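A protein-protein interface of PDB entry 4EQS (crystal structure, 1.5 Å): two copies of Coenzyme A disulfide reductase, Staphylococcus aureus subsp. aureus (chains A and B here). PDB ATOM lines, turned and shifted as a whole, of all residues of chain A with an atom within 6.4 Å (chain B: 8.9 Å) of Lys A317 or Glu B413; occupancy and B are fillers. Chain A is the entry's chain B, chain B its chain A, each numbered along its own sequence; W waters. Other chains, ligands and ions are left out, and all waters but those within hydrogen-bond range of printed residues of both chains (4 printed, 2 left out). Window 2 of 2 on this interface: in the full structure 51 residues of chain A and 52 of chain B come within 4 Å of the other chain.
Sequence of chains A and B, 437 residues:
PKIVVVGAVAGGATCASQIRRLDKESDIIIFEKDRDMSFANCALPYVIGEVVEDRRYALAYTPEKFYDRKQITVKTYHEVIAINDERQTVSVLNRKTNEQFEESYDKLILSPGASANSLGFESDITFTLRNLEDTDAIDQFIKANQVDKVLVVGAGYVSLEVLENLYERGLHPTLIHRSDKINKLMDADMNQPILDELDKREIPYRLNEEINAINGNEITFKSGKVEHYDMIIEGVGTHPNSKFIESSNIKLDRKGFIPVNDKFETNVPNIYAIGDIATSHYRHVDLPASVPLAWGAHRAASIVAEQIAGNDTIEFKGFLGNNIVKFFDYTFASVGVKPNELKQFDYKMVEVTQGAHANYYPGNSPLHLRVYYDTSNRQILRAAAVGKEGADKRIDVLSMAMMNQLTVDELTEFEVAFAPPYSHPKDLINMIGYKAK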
ATOM      1  N   ASP A 262      -8.594  -5.617  13.017  1.00  0.00           N
ATOM      2  CA  ASP A 262      -9.689  -4.814  13.554  1.00  0.00           C
ATOM      3  C   ASP A 262     -11.063  -5.257  13.058  1.00  0.00           C
ATOM      4  O   ASP A 262     -12.083  -4.739  13.504  1.00  0.00           O
ATOM      5  CB  ASP A 262      -9.464  -3.326  13.278  1.00  0.00           C
ATOM      6  CG  ASP A 262      -8.329  -2.747  14.097  1.00  0.00           C
ATOM      7  OD1 ASP A 262      -7.954  -3.354  15.120  1.00  0.00           O
ATOM      8  OD2 ASP A 262      -7.812  -1.677  13.718  1.00  0.00           O
ATOM      9  N   SER A 280      -5.771  -8.310  20.456  1.00  0.00           N
ATOM     10  CA  SER A 280      -5.857  -7.129  19.627  1.00  0.00           C
ATOM     11  C   SER A 280      -4.816  -6.132  20.138  1.00  0.00           C
ATOM     12  O   SER A 280      -3.683  -6.522  20.441  1.00  0.00           O
ATOM     13  CB  SER A 280      -7.279  -6.568  19.699  1.00  0.00           C
ATOM     14  OG  SER A 280      -7.450  -5.426  18.881  1.00  0.00           O
ATOM     15  N   HIS A 281      -5.193  -4.862  20.241  1.00  0.00           N
ATOM     16  CA  HIS A 281      -4.281  -3.810  20.681  1.00  0.00           C
ATOM     17  C   HIS A 281      -5.056  -2.805  21.521  1.00  0.00           C
ATOM     18  O   HIS A 281      -6.282  -2.771  21.471  1.00  0.00           O
ATOM     19  CB  HIS A 281      -3.692  -3.092  19.469  1.00  0.00           C
ATOM     20  CG  HIS A 281      -4.731  -2.563  18.532  1.00  0.00           C
ATOM     21  ND1 HIS A 281      -5.262  -1.298  18.647  1.00  0.00           N
ATOM     22  CD2 HIS A 281      -5.360  -3.142  17.480  1.00  0.00           C
ATOM     23  CE1 HIS A 281      -6.167  -1.113  17.702  1.00  0.00           C
ATOM     24  NE2 HIS A 281      -6.246  -2.218  16.981  1.00  0.00           N
ATOM     25  N   TYR A 282      -4.339  -1.996  22.290  1.00  0.00           N
ATOM     26  CA  TYR A 282      -4.966  -0.883  22.993  1.00  0.00           C
ATOM     27  C   TYR A 282      -5.444   0.180  22.013  1.00  0.00           C
ATOM     28  O   TYR A 282      -4.874   0.362  20.932  1.00  0.00           O
ATOM     29  CB  TYR A 282      -4.004  -0.266  24.008  1.00  0.00           C
ATOM     30  CG  TYR A 282      -3.828  -1.074  25.278  1.00  0.00           C
ATOM     31  CD1 TYR A 282      -2.637  -1.743  25.540  1.00  0.00           C
ATOM     32  CD2 TYR A 282      -4.848  -1.166  26.214  1.00  0.00           C
ATOM     33  CE1 TYR A 282      -2.468  -2.482  26.700  1.00  0.00           C
ATOM     34  CE2 TYR A 282      -4.688  -1.900  27.384  1.00  0.00           C
ATOM     35  CZ  TYR A 282      -3.493  -2.558  27.618  1.00  0.00           C
ATOM     36  OH  TYR A 282      -3.319  -3.281  28.774  1.00  0.00           O
ATOM     37  N   ARG A 283      -6.499   0.889  22.401  1.00  0.00           N
ATOM     38  CA  ARG A 283      -7.017   1.981  21.593  1.00  0.00           C
ATOM     39  C   ARG A 283      -6.153   3.232  21.737  1.00  0.00           C
ATOM     40  O   ARG A 283      -5.970   3.980  20.777  1.00  0.00           O
ATOM     41  CB  ARG A 283      -8.470   2.298  21.975  1.00  0.00           C
ATOM     42  CG  ARG A 283      -9.000   3.548  21.301  1.00  0.00           C
ATOM     43  CD  ARG A 283     -10.500   3.716  21.464  1.00  0.00           C
ATOM     44  NE  ARG A 283     -10.948   4.876  20.692  1.00  0.00           N
ATOM     45  CZ  ARG A 283     -12.168   5.036  20.191  1.00  0.00           C
ATOM     46  NH1 ARG A 283     -13.101   4.118  20.369  1.00  0.00           N
ATOM     47  NH2 ARG A 283     -12.457   6.128  19.496  1.00  0.00           N
ATOM     48  N   HIS A 284      -5.603   3.444  22.928  1.00  0.00           N
ATOM     49  CA  HIS A 284      -4.972   4.722  23.245  1.00  0.00           C
ATOM     50  C   HIS A 284      -3.449   4.699  23.164  1.00  0.00           C
ATOM     51  O   HIS A 284      -2.808   5.754  23.146  1.00  0.00           O
ATOM     52  CB  HIS A 284      -5.427   5.212  24.621  1.00  0.00           C
ATOM     53  CG  HIS A 284      -4.975   4.349  25.758  1.00  0.00           C
ATOM     54  ND1 HIS A 284      -5.034   2.971  25.723  1.00  0.00           N
ATOM     55  CD2 HIS A 284      -4.480   4.671  26.977  1.00  0.00           C
ATOM     56  CE1 HIS A 284      -4.576   2.483  26.860  1.00  0.00           C
ATOM     57  NE2 HIS A 284      -4.238   3.494  27.642  1.00  0.00           N
ATOM     58  N   TRP A 295     -17.539  -7.124  27.959  1.00  0.00           N
ATOM     59  CA  TRP A 295     -17.737  -6.012  27.035  1.00  0.00           C
ATOM     60  C   TRP A 295     -17.103  -6.313  25.686  1.00  0.00           C
ATOM     61  O   TRP A 295     -17.707  -6.067  24.641  1.00  0.00           O
ATOM     62  CB  TRP A 295     -17.180  -4.687  27.584  1.00  0.00           C
ATOM     63  CG  TRP A 295     -17.391  -3.550  26.622  1.00  0.00           C
ATOM     64  CD1 TRP A 295     -18.480  -2.731  26.550  1.00  0.00           C
ATOM     65  CD2 TRP A 295     -16.507  -3.135  25.573  1.00  0.00           C
ATOM     66  NE1 TRP A 295     -18.322  -1.824  25.531  1.00  0.00           N
ATOM     67  CE2 TRP A 295     -17.120  -2.047  24.919  1.00  0.00           C
ATOM     68  CE3 TRP A 295     -15.249  -3.560  25.142  1.00  0.00           C
ATOM     69  CZ2 TRP A 295     -16.521  -1.395  23.836  1.00  0.00           C
ATOM     70  CZ3 TRP A 295     -14.658  -2.914  24.071  1.00  0.00           C
ATOM     71  CH2 TRP A 295     -15.294  -1.843  23.431  1.00  0.00           C
ATOM     72  N   ARG A 299     -18.792  -6.604  22.098  1.00  0.00           N
ATOM     73  CA  ARG A 299     -18.467  -5.632  21.059  1.00  0.00           C
ATOM     74  C   ARG A 299     -17.947  -6.347  19.808  1.00  0.00           C
ATOM     75  O   ARG A 299     -18.351  -6.031  18.685  1.00  0.00           O
ATOM     76  CB  ARG A 299     -17.456  -4.603  21.579  1.00  0.00           C
ATOM     77  CG  ARG A 299     -17.024  -3.565  20.542  1.00  0.00           C
ATOM     78  CD  ARG A 299     -18.198  -2.698  20.078  1.00  0.00           C
ATOM     79  NE  ARG A 299     -17.811  -1.866  18.943  1.00  0.00           N
ATOM     80  CZ  ARG A 299     -18.633  -1.495  17.970  1.00  0.00           C
ATOM     81  NH1 ARG A 299     -18.180  -0.750  16.955  1.00  0.00           N
ATOM     82  NH2 ARG A 299     -19.902  -1.879  18.000  1.00  0.00           N
ATOM     83  N   ILE A 303     -19.306  -6.396  15.866  1.00  0.00           N
ATOM     84  CA  ILE A 303     -18.444  -6.042  14.742  1.00  0.00           C
ATOM     85  C   ILE A 303     -18.368  -7.180  13.721  1.00  0.00           C
ATOM     86  O   ILE A 303     -18.472  -6.950  12.516  1.00  0.00           O
ATOM     87  CB  ILE A 303     -17.041  -5.625  15.215  1.00  0.00           C
ATOM     88  CG1 ILE A 303     -17.121  -4.319  16.012  1.00  0.00           C
ATOM     89  CG2 ILE A 303     -16.105  -5.453  14.031  1.00  0.00           C
ATOM     90  CD1 ILE A 303     -15.808  -3.933  16.685  1.00  0.00           C
ATOM     91  N   GLU A 315     -15.185  -1.198  12.115  1.00  0.00           N
ATOM     92  CA  GLU A 315     -14.018  -1.908  12.620  1.00  0.00           C
ATOM     93  C   GLU A 315     -13.723  -1.543  14.067  1.00  0.00           C
ATOM     94  O   GLU A 315     -14.071  -0.454  14.538  1.00  0.00           O
ATOM     95  CB  GLU A 315     -12.782  -1.629  11.752  1.00  0.00           C
ATOM     96  CG  GLU A 315     -12.919  -2.103  10.312  1.00  0.00           C
ATOM     97  CD  GLU A 315     -11.608  -2.069   9.539  1.00  0.00           C
ATOM     98  OE1 GLU A 315     -10.529  -1.978  10.165  1.00  0.00           O
ATOM     99  OE2 GLU A 315     -11.661  -2.140   8.292  1.00  0.00           O
ATOM    100  N   PHE A 316     -13.087  -2.473  14.769  1.00  0.00           N
ATOM    101  CA  PHE A 316     -12.665  -2.289  16.149  1.00  0.00           C
ATOM    102  C   PHE A 316     -11.642  -1.168  16.213  1.00  0.00           C
ATOM    103  O   PHE A 316     -10.840  -0.997  15.291  1.00  0.00           O
ATOM    104  CB  PHE A 316     -12.027  -3.592  16.634  1.00  0.00           C
ATOM    105  CG  PHE A 316     -11.843  -3.686  18.126  1.00  0.00           C
ATOM    106  CD1 PHE A 316     -12.881  -3.385  18.996  1.00  0.00           C
ATOM    107  CD2 PHE A 316     -10.646  -4.148  18.651  1.00  0.00           C
ATOM    108  CE1 PHE A 316     -12.708  -3.509  20.366  1.00  0.00           C
ATOM    109  CE2 PHE A 316     -10.465  -4.277  20.020  1.00  0.00           C
ATOM    110  CZ  PHE A 316     -11.493  -3.950  20.878  1.00  0.00           C
ATOM    111  N   LYS A 317     -11.661  -0.398  17.294  1.00  0.00           N
ATOM    112  CA  LYS A 317     -10.652   0.637  17.464  1.00  0.00           C
ATOM    113  C   LYS A 317      -9.672   0.335  18.599  1.00  0.00           C
ATOM    114  O   LYS A 317      -8.846   1.176  18.950  1.00  0.00           O
ATOM    115  CB  LYS A 317     -11.306   2.013  17.621  1.00  0.00           C
ATOM    116  CG  LYS A 317     -11.892   2.518  16.306  1.00  0.00           C
ATOM    117  CD  LYS A 317     -12.758   3.743  16.471  1.00  0.00           C
ATOM    118  CE  LYS A 317     -13.328   4.161  15.122  1.00  0.00           C
ATOM    119  NZ  LYS A 317     -14.435   5.146  15.259  1.00  0.00           N
ATOM    120  N   GLY A 318      -9.748  -0.873  19.152  1.00  0.00           N
ATOM    121  CA  GLY A 318      -8.834  -1.271  20.207  1.00  0.00           C
ATOM    122  C   GLY A 318      -9.480  -1.268  21.579  1.00  0.00           C
ATOM    123  O   GLY A 318     -10.577  -0.720  21.762  1.00  0.00           O
ATOM    124  N   PHE A 319      -8.788  -1.866  22.543  1.00  0.00           N
ATOM    125  CA  PHE A 319      -9.272  -1.971  23.916  1.00  0.00           C
ATOM    126  C   PHE A 319      -8.759  -0.840  24.793  1.00  0.00           C
ATOM    127  O   PHE A 319      -7.663  -0.316  24.572  1.00  0.00           O
ATOM    128  CB  PHE A 319      -8.767  -3.265  24.553  1.00  0.00           C
ATOM    129  CG  PHE A 319      -9.517  -4.487  24.142  1.00  0.00           C
ATOM    130  CD1 PHE A 319      -8.928  -5.424  23.316  1.00  0.00           C
ATOM    131  CD2 PHE A 319     -10.802  -4.717  24.604  1.00  0.00           C
ATOM    132  CE1 PHE A 319      -9.613  -6.567  22.939  1.00  0.00           C
ATOM    133  CE2 PHE A 319     -11.487  -5.860  24.236  1.00  0.00           C
ATOM    134  CZ  PHE A 319     -10.889  -6.782  23.410  1.00  0.00           C
ATOM    135  N   LEU A 320      -9.530  -0.503  25.821  1.00  0.00           N
ATOM    136  CA  LEU A 320      -9.021   0.329  26.905  1.00  0.00           C
ATOM    137  C   LEU A 320      -8.766  -0.488  28.173  1.00  0.00           C
ATOM    138  O   LEU A 320      -8.026  -0.058  29.052  1.00  0.00           O
ATOM    139  CB  LEU A 320      -9.965   1.492  27.198  1.00  0.00           C
ATOM    140  CG  LEU A 320     -10.041   2.508  26.061  1.00  0.00           C
ATOM    141  CD1 LEU A 320     -11.166   3.502  26.349  1.00  0.00           C
ATOM    142  CD2 LEU A 320      -8.709   3.219  25.895  1.00  0.00           C
ATOM    143  N   MET A 403     -10.954   7.498  25.282  1.00  0.00           N
ATOM    144  CA  MET A 403     -11.506   7.246  23.959  1.00  0.00           C
ATOM    145  C   MET A 403     -11.341   8.479  23.066  1.00  0.00           C
ATOM    146  O   MET A 403     -11.225   8.373  21.842  1.00  0.00           O
ATOM    147  CB  MET A 403     -12.997   6.933  24.116  1.00  0.00           C
ATOM    148  CG  MET A 403     -13.605   6.072  23.045  1.00  0.00           C
ATOM    149  SD  MET A 403     -15.399   6.100  23.233  1.00  0.00           S
ATOM    150  CE  MET A 403     -15.824   7.339  22.021  1.00  0.00           C
ATOM    151  N   LEU B 406     -18.542  14.394  20.517  1.00  0.00           N
ATOM    152  CA  LEU B 406     -18.724  13.015  20.085  1.00  0.00           C
ATOM    153  C   LEU B 406     -20.064  12.829  19.375  1.00  0.00           C
ATOM    154  O   LEU B 406     -21.043  13.511  19.684  1.00  0.00           O
ATOM    155  CB  LEU B 406     -18.661  12.074  21.289  1.00  0.00           C
ATOM    156  CG  LEU B 406     -18.508  10.591  20.957  1.00  0.00           C
ATOM    157  CD1 LEU B 406     -17.066  10.295  20.610  1.00  0.00           C
ATOM    158  CD2 LEU B 406     -18.973   9.711  22.111  1.00  0.00           C
ATOM    159  N   THR B 407     -20.105  11.906  18.420  1.00  0.00           N
ATOM    160  CA  THR B 407     -21.356  11.620  17.732  1.00  0.00           C
ATOM    161  C   THR B 407     -22.121  10.498  18.420  1.00  0.00           C
ATOM    162  O   THR B 407     -21.550   9.681  19.150  1.00  0.00           O
ATOM    163  CB  THR B 407     -21.136  11.219  16.266  1.00  0.00           C
ATOM    164  OG1 THR B 407     -20.478   9.947  16.199  1.00  0.00           O
ATOM    165  CG2 THR B 407     -20.309  12.274  15.546  1.00  0.00           C
ATOM    166  N   VAL B 408     -23.419  10.455  18.155  1.00  0.00           N
ATOM    167  CA  VAL B 408     -24.277   9.428  18.735  1.00  0.00           C
ATOM    168  C   VAL B 408     -23.830   8.027  18.315  1.00  0.00           C
ATOM    169  O   VAL B 408     -23.872   7.090  19.106  1.00  0.00           O
ATOM    170  CB  VAL B 408     -25.773   9.686  18.392  1.00  0.00           C
ATOM    171  CG1 VAL B 408     -26.033   9.563  16.892  1.00  0.00           C
ATOM    172  CG2 VAL B 408     -26.687   8.758  19.191  1.00  0.00           C
ATOM    173  N   ASP B 409     -23.359   7.896  17.080  1.00  0.00           N
ATOM    174  CA  ASP B 409     -22.959   6.593  16.573  1.00  0.00           C
ATOM    175  C   ASP B 409     -21.757   6.024  17.318  1.00  0.00           C
ATOM    176  O   ASP B 409     -21.642   4.807  17.486  1.00  0.00           O
ATOM    177  CB  ASP B 409     -22.673   6.690  15.080  1.00  0.00           C
ATOM    178  CG  ASP B 409     -23.815   7.324  14.333  1.00  0.00           C
ATOM    179  OD1 ASP B 409     -24.828   6.632  14.100  1.00  0.00           O
ATOM    180  OD2 ASP B 409     -23.712   8.523  14.008  1.00  0.00           O
ATOM    181  N   GLU B 410     -20.872   6.900  17.781  1.00  0.00           N
ATOM    182  CA  GLU B 410     -19.648   6.453  18.435  1.00  0.00           C
ATOM    183  C   GLU B 410     -19.913   5.920  19.837  1.00  0.00           C
ATOM    184  O   GLU B 410     -19.014   5.372  20.476  1.00  0.00           O
ATOM    185  CB  GLU B 410     -18.621   7.585  18.488  1.00  0.00           C
ATOM    186  CG  GLU B 410     -18.051   7.959  17.115  1.00  0.00           C
ATOM    187  CD  GLU B 410     -17.227   9.227  17.164  1.00  0.00           C
ATOM    188  OE1 GLU B 410     -17.821  10.322  17.268  1.00  0.00           O
ATOM    189  OE2 GLU B 410     -15.984   9.126  17.100  1.00  0.00           O
ATOM    190  N   LEU B 411     -21.141   6.081  20.322  1.00  0.00           N
ATOM    191  CA  LEU B 411     -21.473   5.566  21.643  1.00  0.00           C
ATOM    192  C   LEU B 411     -21.394   4.038  21.685  1.00  0.00           C
ATOM    193  O   LEU B 411     -21.247   3.449  22.761  1.00  0.00           O
ATOM    194  CB  LEU B 411     -22.842   6.078  22.104  1.00  0.00           C
ATOM    195  CG  LEU B 411     -22.930   7.589  22.350  1.00  0.00           C
ATOM    196  CD1 LEU B 411     -24.352   7.980  22.706  1.00  0.00           C
ATOM    197  CD2 LEU B 411     -21.977   8.024  23.460  1.00  0.00           C
ATOM    198  N   THR B 412     -21.482   3.391  20.524  1.00  0.00           N
ATOM    199  CA  THR B 412     -21.320   1.939  20.488  1.00  0.00           C
ATOM    200  C   THR B 412     -19.924   1.516  20.945  1.00  0.00           C
ATOM    201  O   THR B 412     -19.725   0.371  21.371  1.00  0.00           O
ATOM    202  CB  THR B 412     -21.539   1.350  19.070  1.00  0.00           C
ATOM    203  OG1 THR B 412     -20.602   1.932  18.156  1.00  0.00           O
ATOM    204  CG2 THR B 412     -22.959   1.604  18.581  1.00  0.00           C
ATOM    205  N   GLU B 413     -18.976   2.450  20.869  1.00  0.00           N
ATOM    206  CA  GLU B 413     -17.565   2.185  21.138  1.00  0.00           C
ATOM    207  C   GLU B 413     -17.161   2.444  22.587  1.00  0.00           C
ATOM    208  O   GLU B 413     -16.040   2.126  22.984  1.00  0.00           O
ATOM    209  CB  GLU B 413     -16.675   3.041  20.229  1.00  0.00           C
ATOM    210  CG  GLU B 413     -16.924   2.869  18.733  1.00  0.00           C
ATOM    211  CD  GLU B 413     -16.244   3.939  17.912  1.00  0.00           C
ATOM    212  OE1 GLU B 413     -15.390   4.656  18.464  1.00  0.00           O
ATOM    213  OE2 GLU B 413     -16.564   4.070  16.713  1.00  0.00           O
ATOM    214  N   PHE B 414     -18.058   3.056  23.360  1.00  0.00           N
ATOM    215  CA  PHE B 414     -17.780   3.338  24.756  1.00  0.00           C
ATOM    216  C   PHE B 414     -17.551   2.036  25.518  1.00  0.00           C
ATOM    217  O   PHE B 414     -18.399   1.145  25.512  1.00  0.00           O
ATOM    218  CB  PHE B 414     -18.934   4.136  25.370  1.00  0.00           C
ATOM    219  CG  PHE B 414     -18.914   4.173  26.868  1.00  0.00           C
ATOM    220  CD1 PHE B 414     -17.850   4.745  27.548  1.00  0.00           C
ATOM    221  CD2 PHE B 414     -19.965   3.633  27.595  1.00  0.00           C
ATOM    222  CE1 PHE B 414     -17.837   4.774  28.931  1.00  0.00           C
ATOM    223  CE2 PHE B 414     -19.958   3.661  28.980  1.00  0.00           C
ATOM    224  CZ  PHE B 414     -18.892   4.231  29.643  1.00  0.00           C
ATOM    225  N   GLU B 415     -16.396   1.936  26.166  1.00  0.00           N
ATOM    226  CA  GLU B 415     -16.020   0.719  26.872  1.00  0.00           C
ATOM    227  C   GLU B 415     -16.358   0.881  28.346  1.00  0.00           C
ATOM    228  O   GLU B 415     -15.649   1.554  29.097  1.00  0.00           O
ATOM    229  CB  GLU B 415     -14.538   0.406  26.661  1.00  0.00           C
ATOM    230  CG  GLU B 415     -14.128  -0.936  27.249  1.00  0.00           C
ATOM    231  CD  GLU B 415     -12.710  -1.328  26.906  1.00  0.00           C
ATOM    232  OE1 GLU B 415     -12.083  -2.025  27.726  1.00  0.00           O
ATOM    233  OE2 GLU B 415     -12.220  -0.945  25.827  1.00  0.00           O
ATOM    234  N   VAL B 416     -17.474   0.283  28.741  1.00  0.00           N
ATOM    235  CA  VAL B 416     -17.996   0.424  30.092  1.00  0.00           C
ATOM    236  C   VAL B 416     -17.249  -0.478  31.069  1.00  0.00           C
ATOM    237  O   VAL B 416     -16.651  -1.481  30.674  1.00  0.00           O
ATOM    238  CB  VAL B 416     -19.521   0.109  30.121  1.00  0.00           C
ATOM    239  CG1 VAL B 416     -19.776  -1.393  29.951  1.00  0.00           C
ATOM    240  CG2 VAL B 416     -20.175   0.638  31.403  1.00  0.00           C
ATOM    241  N   ILE B 429     -25.622   3.203  27.469  1.00  0.00           N
ATOM    242  CA  ILE B 429     -24.971   4.141  26.559  1.00  0.00           C
ATOM    243  C   ILE B 429     -24.637   3.484  25.215  1.00  0.00           C
ATOM    244  O   ILE B 429     -24.864   4.063  24.147  1.00  0.00           O
ATOM    245  CB  ILE B 429     -23.718   4.748  27.201  1.00  0.00           C
ATOM    246  CG1 ILE B 429     -24.130   5.731  28.298  1.00  0.00           C
ATOM    247  CG2 ILE B 429     -22.869   5.464  26.165  1.00  0.00           C
ATOM    248  CD1 ILE B 429     -22.978   6.242  29.124  1.00  0.00           C
ATOM    249  N   ASN B 430     -24.122   2.257  25.259  1.00  0.00           N
ATOM    250  CA  ASN B 430     -23.874   1.519  24.027  1.00  0.00           C
ATOM    251  C   ASN B 430     -25.163   1.320  23.239  1.00  0.00           C
ATOM    252  O   ASN B 430     -25.185   1.468  22.020  1.00  0.00           O
ATOM    253  CB  ASN B 430     -23.262   0.149  24.329  1.00  0.00           C
ATOM    254  CG  ASN B 430     -21.901   0.235  24.987  1.00  0.00           C
ATOM    255  OD1 ASN B 430     -21.610  -0.512  25.931  1.00  0.00           O
ATOM    256  ND2 ASN B 430     -21.048   1.123  24.487  1.00  0.00           N
ATOM    257  N   MET B 431     -26.247   1.004  23.943  1.00  0.00           N
ATOM    258  CA  MET B 431     -27.513   0.733  23.272  1.00  0.00           C
ATOM    259  C   MET B 431     -28.071   1.954  22.544  1.00  0.00           C
ATOM    260  O   MET B 431     -28.718   1.815  21.507  1.00  0.00           O
ATOM    261  CB  MET B 431     -28.537   0.153  24.248  1.00  0.00           C
ATOM    262  CG  MET B 431     -28.158  -1.228  24.788  1.00  0.00           C
ATOM    263  SD  MET B 431     -27.758  -2.448  23.511  1.00  0.00           S
ATOM    264  CE  MET B 431     -29.165  -2.264  22.417  1.00  0.00           C
ATOM    265  N   ILE B 432     -27.819   3.146  23.078  1.00  0.00           N
ATOM    266  CA  ILE B 432     -28.199   4.370  22.384  1.00  0.00           C
ATOM    267  C   ILE B 432     -27.528   4.381  21.010  1.00  0.00           C
ATOM    268  O   ILE B 432     -28.163   4.667  19.998  1.00  0.00           O
ATOM    269  CB  ILE B 432     -27.803   5.632  23.176  1.00  0.00           C
ATOM    270  CG1 ILE B 432     -28.633   5.747  24.457  1.00  0.00           C
ATOM    271  CG2 ILE B 432     -27.977   6.880  22.312  1.00  0.00           C
ATOM    272  CD1 ILE B 432     -30.061   6.190  24.216  1.00  0.00           C
ATOM    273  N   GLY B 433     -26.241   4.048  20.989  1.00  0.00           N
ATOM    274  CA  GLY B 433     -25.487   4.005  19.751  1.00  0.00           C
ATOM    275  C   GLY B 433     -26.025   2.964  18.785  1.00  0.00           C
ATOM    276  O   GLY B 433     -26.168   3.234  17.596  1.00  0.00           O
ATOM    277  N   TYR B 434     -26.331   1.773  19.285  1.00  0.00           N
ATOM    278  CA  TYR B 434     -26.834   0.718  18.407  1.00  0.00           C
ATOM    279  C   TYR B 434     -28.208   1.065  17.841  1.00  0.00           C
ATOM    280  O   TYR B 434     -28.557   0.647  16.735  1.00  0.00           O
ATOM    281  CB  TYR B 434     -26.876  -0.638  19.125  1.00  0.00           C
ATOM    282  CG  TYR B 434     -25.515  -1.233  19.390  1.00  0.00           C
ATOM    283  CD1 TYR B 434     -25.074  -1.459  20.685  1.00  0.00           C
ATOM    284  CD2 TYR B 434     -24.666  -1.580  18.336  1.00  0.00           C
ATOM    285  CE1 TYR B 434     -23.828  -2.006  20.931  1.00  0.00           C
ATOM    286  CE2 TYR B 434     -23.412  -2.117  18.574  1.00  0.00           C
ATOM    287  CZ  TYR B 434     -23.000  -2.338  19.870  1.00  0.00           C
ATOM    288  OH  TYR B 434     -21.754  -2.877  20.118  1.00  0.00           O
HETATM  289  O   HOH W   1     -14.586   4.208  26.205  1.00  0.00           O
HETATM  290  O   HOH W   2     -20.437   0.863  15.514  1.00  0.00           O
HETATM  291  O   HOH W   3     -12.245   0.548  23.565  1.00  0.00           O
HETATM  292  O   HOH W   4     -14.467   6.809  17.480  1.00  0.00           O
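O of Thr B412 is in hydrogen-bond range of ND2 of Asn B430 (3.5 Å).
The side-chain amide nitrogen (ND2) of Asn B430 lies within hydrogen-bond range of the backbone carbonyl oxygen (O) of Phe B414, at 2.8 Å.
The backbone NH (N) of Arg A283 sits at hydrogen-bond distance from the backbone carbonyl oxygen (O) of Phe A319 (2.7 Å).
The side-chain amide nitrogen (ND2) of Asn B430 lies within hydrogen-bond range of the backbone carbonyl oxygen (O) of Leu B411 (2.9 Å).
The side-chain hydroxyl (OG1) of Thr B412 is in hydrogen-bond range of the backbone carbonyl oxygen (O) of Asp B409, at 3.1 Å.
The guanidinium group (NH2) of Arg A283 is in hydrogen-bond range of the backbone carbonyl oxygen (O) of Met A403, 3.5 Å away.
NZ of Lys A317 lies within salt-bridge range of OE2 of Glu B413 (2.8 Å).
The side-chain hydroxyl of Tyr B434 lies within hydrogen-bond range of the guanidinium group of Arg A299 (3.0 Å).
The side-chain carboxylate (OE1) of Glu B413 is in salt-bridge range of the guanidinium group (NH1) of Arg A283, at 3.0 Å.
N of Leu A320 is in hydrogen-bond range of OE2 of Glu B415 (2.7 Å).
NE1 of Trp A295 lies within hydrogen-bond range of O of Phe B414 (3.0 Å).
Of the 16 printed residues of chain A, 7 touch a printed residue of chain B.
Hydrophobic or aromatic side chains of chain A within 4 Å of the printed part of chain B: Trp A295, Leu A320 and Met A403.
Of the 17 printed residues of chain B, 8 touch a printed residue of chain A.
Among the printed residues, 13 pairs touch across the chains.
Among the printed residues, Asp or Glu carboxylates within 4 Å of a Lys or Arg side-chain nitrogen of the other chain: Arg A283 with Glu B413 and Lys A317 with Glu B413.
Water W4 lies within hydrogen-bond range of OE1 of Glu B413 (2.5 Å), NZ of Lys A317 (2.8 Å), OE2 of Glu B410 (2.8 Å) and NH2 of Arg A283 (2.9 Å).
Water W3 bridges OE2 of Glu B415 (2.7 Å) and O of Gly A318 (2.8 Å).
Water W2 bridges OG1 of Thr B412 and NH1 of Arg A299.
Water W1 lies within hydrogen-bond range of the backbone NH of Glu B415 (2.9 Å) and the side-chain sulfur of Met A403 (3.6 Å).
Lys A317 touches just one residue of chain B: Glu B413.
Of chain A, only Arg A283 (3.0 Å), Trp A295 (3.7 Å) and Lys A317 (2.8 Å) come within 4 Å of Glu B413.
Of chain B, only Glu B413 (3.0 Å) comes within 4 Å of Arg A283.
No residue of chain B comes within 4 Å of Gly A318.
Printed residues of chain B within 4 Å of Phe A319: Glu B415 (3.6 Å).
Printed residues of chain A within 4 Å of Leu B406: Met A403.
Phe A316 touches none of the printed residues of chain B.
Ser A280 touches none of the printed residues of chain B.
The nearest residue of chain B that does not touch Lys A317 is Glu B410 (4.7 Å).
Among the printed residues, merely in contact across the chains: Met A403 with Leu B406, Trp A295 with Glu B415, Trp A295 with Asn B430, Phe A319 with Glu B415, Trp A295 with Glu B413, Arg A299 with Thr B412, Trp A295 with Val B416 and Met A403 with Phe B414.
No position is printed for both chains.
Of the 13 pairs that touch across the chains among the printed residues, none has its exchanged pair printed and touching as well.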
